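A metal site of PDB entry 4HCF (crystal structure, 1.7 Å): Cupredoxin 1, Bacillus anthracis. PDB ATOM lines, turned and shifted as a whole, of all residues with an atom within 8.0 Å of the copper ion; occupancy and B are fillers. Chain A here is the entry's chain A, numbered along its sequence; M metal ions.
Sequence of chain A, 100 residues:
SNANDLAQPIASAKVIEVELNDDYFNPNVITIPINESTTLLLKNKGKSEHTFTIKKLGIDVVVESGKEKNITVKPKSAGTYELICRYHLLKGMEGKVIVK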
ATOM      1  N   LEU A  20     -27.825  35.099  27.331  1.00  0.00           N
ATOM      2  CA  LEU A  20     -27.012  33.923  26.991  1.00  0.00           C
ATOM      3  C   LEU A  20     -25.614  34.441  26.612  1.00  0.00           C
ATOM      4  O   LEU A  20     -25.465  35.087  25.588  1.00  0.00           O
ATOM      5  CB  LEU A  20     -27.622  33.135  25.833  1.00  0.00           C
ATOM      6  CG  LEU A  20     -28.955  32.422  26.121  1.00  0.00           C
ATOM      7  CD1 LEU A  20     -30.124  33.401  26.166  1.00  0.00           C
ATOM      8  CD2 LEU A  20     -29.226  31.350  25.075  1.00  0.00           C
ATOM      9  N   ASN A  21     -24.613  34.168  27.446  1.00  0.00           N
ATOM     10  CA  ASN A  21     -23.270  34.691  27.231  1.00  0.00           C
ATOM     11  C   ASN A  21     -22.332  33.540  26.928  1.00  0.00           C
ATOM     12  O   ASN A  21     -22.714  32.398  27.104  1.00  0.00           O
ATOM     13  CB  ASN A  21     -22.765  35.389  28.508  1.00  0.00           C
ATOM     14  CG  ASN A  21     -23.608  36.604  28.900  1.00  0.00           C
ATOM     15  OD1 ASN A  21     -23.791  37.525  28.106  1.00  0.00           O
ATOM     16  ND2 ASN A  21     -24.144  36.598  30.107  1.00  0.00           N
ATOM     17  N   ASP A  22     -21.106  33.832  26.505  1.00  0.00           N
ATOM     18  CA  ASP A  22     -20.110  32.778  26.332  1.00  0.00           C
ATOM     19  C   ASP A  22     -19.421  32.511  27.697  1.00  0.00           C
ATOM     20  O   ASP A  22     -18.724  33.397  28.166  1.00  0.00           O
ATOM     21  CB  ASP A  22     -19.008  33.245  25.371  1.00  0.00           C
ATOM     22  CG  ASP A  22     -19.528  33.618  23.976  1.00  0.00           C
ATOM     23  OD1 ASP A  22     -20.593  33.133  23.541  1.00  0.00           O
ATOM     24  OD2 ASP A  22     -18.825  34.398  23.292  1.00  0.00           O
ATOM     25  N   ASP A  23     -19.604  31.361  28.355  1.00  0.00           N
ATOM     26  CA  ASP A  23     -20.613  30.331  28.086  1.00  0.00           C
ATOM     27  C   ASP A  23     -21.372  30.137  29.387  1.00  0.00           C
ATOM     28  O   ASP A  23     -21.143  29.161  30.121  1.00  0.00           O
ATOM     29  CB  ASP A  23     -19.943  29.000  27.742  1.00  0.00           C
ATOM     30  CG  ASP A  23     -19.226  29.018  26.404  1.00  0.00           C
ATOM     31  OD1 ASP A  23     -18.221  28.286  26.284  1.00  0.00           O
ATOM     32  OD2 ASP A  23     -19.676  29.721  25.488  1.00  0.00           O
ATOM     33  N   TYR A  24     -22.270  31.064  29.698  1.00  0.00           N
ATOM     34  CA  TYR A  24     -23.100  30.935  30.902  1.00  0.00           C
ATOM     35  C   TYR A  24     -24.413  31.646  30.722  1.00  0.00           C
ATOM     36  O   TYR A  24     -24.535  32.497  29.827  1.00  0.00           O
ATOM     37  CB  TYR A  24     -22.345  31.526  32.097  1.00  0.00           C
ATOM     38  CG  TYR A  24     -22.034  33.010  32.011  1.00  0.00           C
ATOM     39  CD1 TYR A  24     -20.898  33.469  31.344  1.00  0.00           C
ATOM     40  CD2 TYR A  24     -22.828  33.944  32.666  1.00  0.00           C
ATOM     41  CE1 TYR A  24     -20.595  34.821  31.297  1.00  0.00           C
ATOM     42  CE2 TYR A  24     -22.520  35.309  32.617  1.00  0.00           C
ATOM     43  CZ  TYR A  24     -21.409  35.730  31.933  1.00  0.00           C
ATOM     44  OH  TYR A  24     -21.099  37.071  31.888  1.00  0.00           O
ATOM     45  N   PHE A  25     -25.387  31.313  31.567  1.00  0.00           N
ATOM     46  CA  PHE A  25     -26.660  32.017  31.610  1.00  0.00           C
ATOM     47  C   PHE A  25     -26.635  33.071  32.701  1.00  0.00           C
ATOM     48  O   PHE A  25     -26.062  32.867  33.781  1.00  0.00           O
ATOM     49  CB  PHE A  25     -27.823  31.055  31.886  1.00  0.00           C
ATOM     50  CG  PHE A  25     -28.012  30.011  30.817  1.00  0.00           C
ATOM     51  CD1 PHE A  25     -28.633  30.346  29.621  1.00  0.00           C
ATOM     52  CD2 PHE A  25     -27.592  28.695  30.998  1.00  0.00           C
ATOM     53  CE1 PHE A  25     -28.844  29.406  28.635  1.00  0.00           C
ATOM     54  CE2 PHE A  25     -27.802  27.749  30.024  1.00  0.00           C
ATOM     55  CZ  PHE A  25     -28.424  28.098  28.820  1.00  0.00           C
ATOM     56  N   ASN A  44     -28.906  36.666  23.265  1.00  0.00           N
ATOM     57  CA  ASN A  44     -27.568  36.095  23.118  1.00  0.00           C
ATOM     58  C   ASN A  44     -26.575  37.236  22.954  1.00  0.00           C
ATOM     59  O   ASN A  44     -26.540  37.885  21.905  1.00  0.00           O
ATOM     60  CB  ASN A  44     -27.483  35.147  21.922  1.00  0.00           C
ATOM     61  CG  ASN A  44     -26.094  34.489  21.778  1.00  0.00           C
ATOM     62  OD1 ASN A  44     -25.119  34.968  22.348  1.00  0.00           O
ATOM     63  ND2 ASN A  44     -26.020  33.413  21.024  1.00  0.00           N
ATOM     64  N   SER A  48     -20.795  33.168  20.195  1.00  0.00           N
ATOM     65  CA  SER A  48     -21.161  31.814  19.756  1.00  0.00           C
ATOM     66  C   SER A  48     -22.670  31.686  19.685  1.00  0.00           C
ATOM     67  O   SER A  48     -23.392  32.433  20.323  1.00  0.00           O
ATOM     68  CB  SER A  48     -20.638  30.765  20.753  1.00  0.00           C
ATOM     69  OG  SER A  48     -19.218  30.782  20.855  1.00  0.00           O
ATOM     70  N   GLU A  49     -23.145  30.714  18.903  1.00  0.00           N
ATOM     71  CA  GLU A  49     -24.548  30.282  18.969  1.00  0.00           C
ATOM     72  C   GLU A  49     -24.799  29.550  20.289  1.00  0.00           C
ATOM     73  O   GLU A  49     -23.932  28.792  20.770  1.00  0.00           O
ATOM     74  CB  GLU A  49     -24.839  29.340  17.790  1.00  0.00           C
ATOM     75  CG  GLU A  49     -26.283  28.863  17.711  1.00  0.00           C
ATOM     76  CD  GLU A  49     -26.533  27.934  16.536  1.00  0.00           C
ATOM     77  OE1 GLU A  49     -26.250  26.725  16.635  1.00  0.00           O
ATOM     78  OE2 GLU A  49     -27.008  28.413  15.480  1.00  0.00           O
ATOM     79  N   HIS A  50     -25.966  29.775  20.896  1.00  0.00           N
ATOM     80  CA  HIS A  50     -26.303  29.116  22.169  1.00  0.00           C
ATOM     81  C   HIS A  50     -27.712  28.573  22.119  1.00  0.00           C
ATOM     82  O   HIS A  50     -28.520  28.995  21.307  1.00  0.00           O
ATOM     83  CB  HIS A  50     -26.185  30.100  23.347  1.00  0.00           C
ATOM     84  CG  HIS A  50     -24.783  30.592  23.593  1.00  0.00           C
ATOM     85  ND1 HIS A  50     -23.769  29.760  23.998  1.00  0.00           N
ATOM     86  CD2 HIS A  50     -24.245  31.835  23.511  1.00  0.00           C
ATOM     87  CE1 HIS A  50     -22.648  30.450  24.112  1.00  0.00           C
ATOM     88  NE2 HIS A  50     -22.909  31.712  23.817  1.00  0.00           N
ATOM     89  N   THR A  51     -28.038  27.640  23.015  1.00  0.00           N
ATOM     90  CA  THR A  51     -29.428  27.247  23.209  1.00  0.00           C
ATOM     91  C   THR A  51     -29.929  27.464  24.625  1.00  0.00           C
ATOM     92  O   THR A  51     -29.146  27.597  25.574  1.00  0.00           O
ATOM     93  CB  THR A  51     -29.704  25.760  22.804  1.00  0.00           C
ATOM     94  OG1 THR A  51     -29.321  24.871  23.886  1.00  0.00           O
ATOM     95  CG2 THR A  51     -28.939  25.397  21.547  1.00  0.00           C
ATOM     96  N   PHE A  52     -31.244  27.504  24.742  1.00  0.00           N
ATOM     97  CA  PHE A  52     -31.923  27.609  26.019  1.00  0.00           C
ATOM     98  C   PHE A  52     -32.833  26.387  26.021  1.00  0.00           C
ATOM     99  O   PHE A  52     -33.856  26.365  25.352  1.00  0.00           O
ATOM    100  CB  PHE A  52     -32.736  28.909  26.057  1.00  0.00           C
ATOM    101  CG  PHE A  52     -33.407  29.183  27.376  1.00  0.00           C
ATOM    102  CD1 PHE A  52     -32.728  29.876  28.397  1.00  0.00           C
ATOM    103  CD2 PHE A  52     -34.726  28.789  27.582  1.00  0.00           C
ATOM    104  CE1 PHE A  52     -33.351  30.149  29.610  1.00  0.00           C
ATOM    105  CE2 PHE A  52     -35.355  29.041  28.793  1.00  0.00           C
ATOM    106  CZ  PHE A  52     -34.682  29.727  29.803  1.00  0.00           C
ATOM    107  N   VAL A  63     -30.609  30.346  19.852  1.00  0.00           N
ATOM    108  CA  VAL A  63     -30.480  31.799  19.683  1.00  0.00           C
ATOM    109  C   VAL A  63     -29.109  32.097  19.089  1.00  0.00           C
ATOM    110  O   VAL A  63     -28.076  31.832  19.729  1.00  0.00           O
ATOM    111  CB  VAL A  63     -30.616  32.536  21.031  1.00  0.00           C
ATOM    112  CG1 VAL A  63     -30.728  34.061  20.792  1.00  0.00           C
ATOM    113  CG2 VAL A  63     -31.859  32.023  21.789  1.00  0.00           C
ATOM    114  N   ILE A  84     -30.062  23.764  30.212  1.00  0.00           N
ATOM    115  CA  ILE A  84     -28.750  23.579  29.592  1.00  0.00           C
ATOM    116  C   ILE A  84     -28.641  24.322  28.270  1.00  0.00           C
ATOM    117  O   ILE A  84     -29.652  24.670  27.670  1.00  0.00           O
ATOM    118  CB  ILE A  84     -28.454  22.076  29.335  1.00  0.00           C
ATOM    119  CG1 ILE A  84     -29.340  21.533  28.202  1.00  0.00           C
ATOM    120  CG2 ILE A  84     -28.656  21.249  30.606  1.00  0.00           C
ATOM    121  CD1 ILE A  84     -28.878  20.182  27.663  1.00  0.00           C
ATOM    122  N   CYS A  85     -27.408  24.602  27.849  1.00  0.00           N
ATOM    123  CA  CYS A  85     -27.126  24.878  26.440  1.00  0.00           C
ATOM    124  C   CYS A  85     -26.563  23.592  25.873  1.00  0.00           C
ATOM    125  O   CYS A  85     -25.591  23.027  26.386  1.00  0.00           O
ATOM    126  CB  CYS A  85     -26.102  25.987  26.275  1.00  0.00           C
ATOM    127  SG  CYS A  85     -25.467  26.151  24.580  1.00  0.00           S
ATOM    128  N   ARG A  86     -27.171  23.134  24.796  1.00  0.00           N
ATOM    129  CA  ARG A  86     -26.773  21.865  24.191  1.00  0.00           C
ATOM    130  C   ARG A  86     -25.339  21.931  23.670  1.00  0.00           C
ATOM    131  O   ARG A  86     -24.697  20.883  23.520  1.00  0.00           O
ATOM    132  CB  ARG A  86     -27.698  21.517  23.020  1.00  0.00           C
ATOM    133  CG  ARG A  86     -29.078  20.958  23.393  1.00  0.00           C
ATOM    134  CD  ARG A  86     -29.678  20.211  22.177  1.00  0.00           C
ATOM    135  NE  ARG A  86     -31.122  20.014  22.257  1.00  0.00           N
ATOM    136  CZ  ARG A  86     -31.693  18.888  22.711  1.00  0.00           C
ATOM    137  NH1 ARG A  86     -30.934  17.886  23.127  1.00  0.00           N
ATOM    138  NH2 ARG A  86     -33.018  18.784  22.735  1.00  0.00           N
ATOM    139  N   TYR A  87     -24.849  23.130  23.373  1.00  0.00           N
ATOM    140  CA  TYR A  87     -23.542  23.253  22.738  1.00  0.00           C
ATOM    141  C   TYR A  87     -22.408  23.355  23.738  1.00  0.00           C
ATOM    142  O   TYR A  87     -21.300  22.890  23.475  1.00  0.00           O
ATOM    143  CB  TYR A  87     -23.525  24.470  21.824  1.00  0.00           C
ATOM    144  CG  TYR A  87     -24.572  24.407  20.735  1.00  0.00           C
ATOM    145  CD1 TYR A  87     -24.903  23.200  20.138  1.00  0.00           C
ATOM    146  CD2 TYR A  87     -25.243  25.547  20.350  1.00  0.00           C
ATOM    147  CE1 TYR A  87     -25.863  23.137  19.154  1.00  0.00           C
ATOM    148  CE2 TYR A  87     -26.204  25.495  19.388  1.00  0.00           C
ATOM    149  CZ  TYR A  87     -26.515  24.302  18.788  1.00  0.00           C
ATOM    150  OH  TYR A  87     -27.492  24.274  17.822  1.00  0.00           O
ATOM    151  N   HIS A  88     -22.693  23.978  24.882  1.00  0.00           N
ATOM    152  CA  HIS A  88     -21.646  24.276  25.857  1.00  0.00           C
ATOM    153  C   HIS A  88     -21.929  23.756  27.265  1.00  0.00           C
ATOM    154  O   HIS A  88     -21.284  24.186  28.223  1.00  0.00           O
ATOM    155  CB  HIS A  88     -21.369  25.776  25.915  1.00  0.00           C
ATOM    156  CG  HIS A  88     -21.115  26.381  24.557  1.00  0.00           C
ATOM    157  ND1 HIS A  88     -22.000  27.257  23.969  1.00  0.00           N
ATOM    158  CD2 HIS A  88     -20.092  26.229  23.686  1.00  0.00           C
ATOM    159  CE1 HIS A  88     -21.530  27.615  22.787  1.00  0.00           C
ATOM    160  NE2 HIS A  88     -20.367  27.009  22.593  1.00  0.00           N
ATOM    161  N   LEU A  89     -22.884  22.837  27.393  1.00  0.00           N
ATOM    162  CA  LEU A  89     -23.159  22.207  28.684  1.00  0.00           C
ATOM    163  C   LEU A  89     -21.881  21.738  29.369  1.00  0.00           C
ATOM    164  O   LEU A  89     -21.692  21.972  30.565  1.00  0.00           O
ATOM    165  CB  LEU A  89     -24.087  20.995  28.504  1.00  0.00           C
ATOM    166  CG  LEU A  89     -24.338  20.158  29.764  1.00  0.00           C
ATOM    167  CD1 LEU A  89     -24.965  21.047  30.859  1.00  0.00           C
ATOM    168  CD2 LEU A  89     -25.234  18.972  29.445  1.00  0.00           C
ATOM    169  N   LYS A  91     -18.989  22.764  29.310  1.00  0.00           N
ATOM    170  CA  LYS A  91     -18.183  23.886  29.792  1.00  0.00           C
ATOM    171  C   LYS A  91     -18.853  24.609  30.966  1.00  0.00           C
ATOM    172  O   LYS A  91     -18.335  25.610  31.469  1.00  0.00           O
ATOM    173  CB  LYS A  91     -17.902  24.878  28.652  1.00  0.00           C
ATOM    174  CG  LYS A  91     -17.063  24.256  27.524  1.00  0.00           C
ATOM    175  CD  LYS A  91     -16.831  25.238  26.374  1.00  0.00           C
ATOM    176  CE  LYS A  91     -15.585  26.071  26.605  1.00  0.00           C
ATOM    177  NZ  LYS A  91     -15.155  26.804  25.379  1.00  0.00           N
ATOM    178  N   MET A  93     -22.230  25.507  30.938  1.00  0.00           N
ATOM    179  CA  MET A  93     -23.365  26.342  30.533  1.00  0.00           C
ATOM    180  C   MET A  93     -24.673  25.680  30.923  1.00  0.00           C
ATOM    181  O   MET A  93     -25.309  24.937  30.151  1.00  0.00           O
ATOM    182  CB  MET A  93     -23.313  26.713  29.050  1.00  0.00           C
ATOM    183  CG  MET A  93     -24.310  27.853  28.682  1.00  0.00           C
ATOM    184  SD  MET A  93     -23.781  28.784  27.113  1.00  0.00           S
ATOM    185  CE  MET A  93     -25.191  30.150  27.036  1.00  0.00           C
ATOM    186  N   GLU A  94     -25.059  25.925  32.165  1.00  0.00           N
ATOM    187  CA  GLU A  94     -26.131  25.208  32.798  1.00  0.00           C
ATOM    188  C   GLU A  94     -26.758  26.084  33.871  1.00  0.00           C
ATOM    189  O   GLU A  94     -26.110  26.986  34.437  1.00  0.00           O
ATOM    190  CB  GLU A  94     -25.558  23.935  33.440  1.00  0.00           C
ATOM    191  CG  GLU A  94     -26.587  22.936  33.926  1.00  0.00           C
ATOM    192  CD  GLU A  94     -26.482  22.720  35.413  1.00  0.00           C
ATOM    193  OE1 GLU A  94     -25.855  23.554  36.088  1.00  0.00           O
ATOM    194  OE2 GLU A  94     -27.035  21.719  35.911  1.00  0.00           O
HETATM  195 CU    CU M   1     -23.957  27.765  24.694  1.00  0.00          CU
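The backbone carbonyl oxygen (O) of Asn 21 is in hydrogen-bond range of a ring nitrogen (NE2) of His 50 (3.4 Å). A ring nitrogen (NE2) of His 50 is in hydrogen-bond range of the side-chain carboxylate (OD1) of Asp 22, 2.7 Å away. The backbone carbonyl oxygen (O) of His 50 is in hydrogen-bond range of the backbone NH (N) of Val 63 (2.9 Å). SG of Cys 85 lies close to N of Tyr 87. The backbone NH (N) of Thr 51 sits close to the side-chain sulfur (SG) of Cys 85 (3.4 Å). The side-chain sulfur of Met 93 sits close to the backbone NH of Tyr 24 (3.8 Å).
Four residues have an atom within 4 Å of the copper ion: His 50, Cys 85, His 88 and Met 93. Along chain A the residues within 4 Å of the copper ion span positions 50 to 93.
The copper ion is bound by ND1 of His 50 (2.1 Å). The copper ion is bound by a ring nitrogen (ND1) of His 88 (2.1 Å). The copper ion is bound by SG of Cys 85. SD of Met 93 binds the copper ion (2.6 Å).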
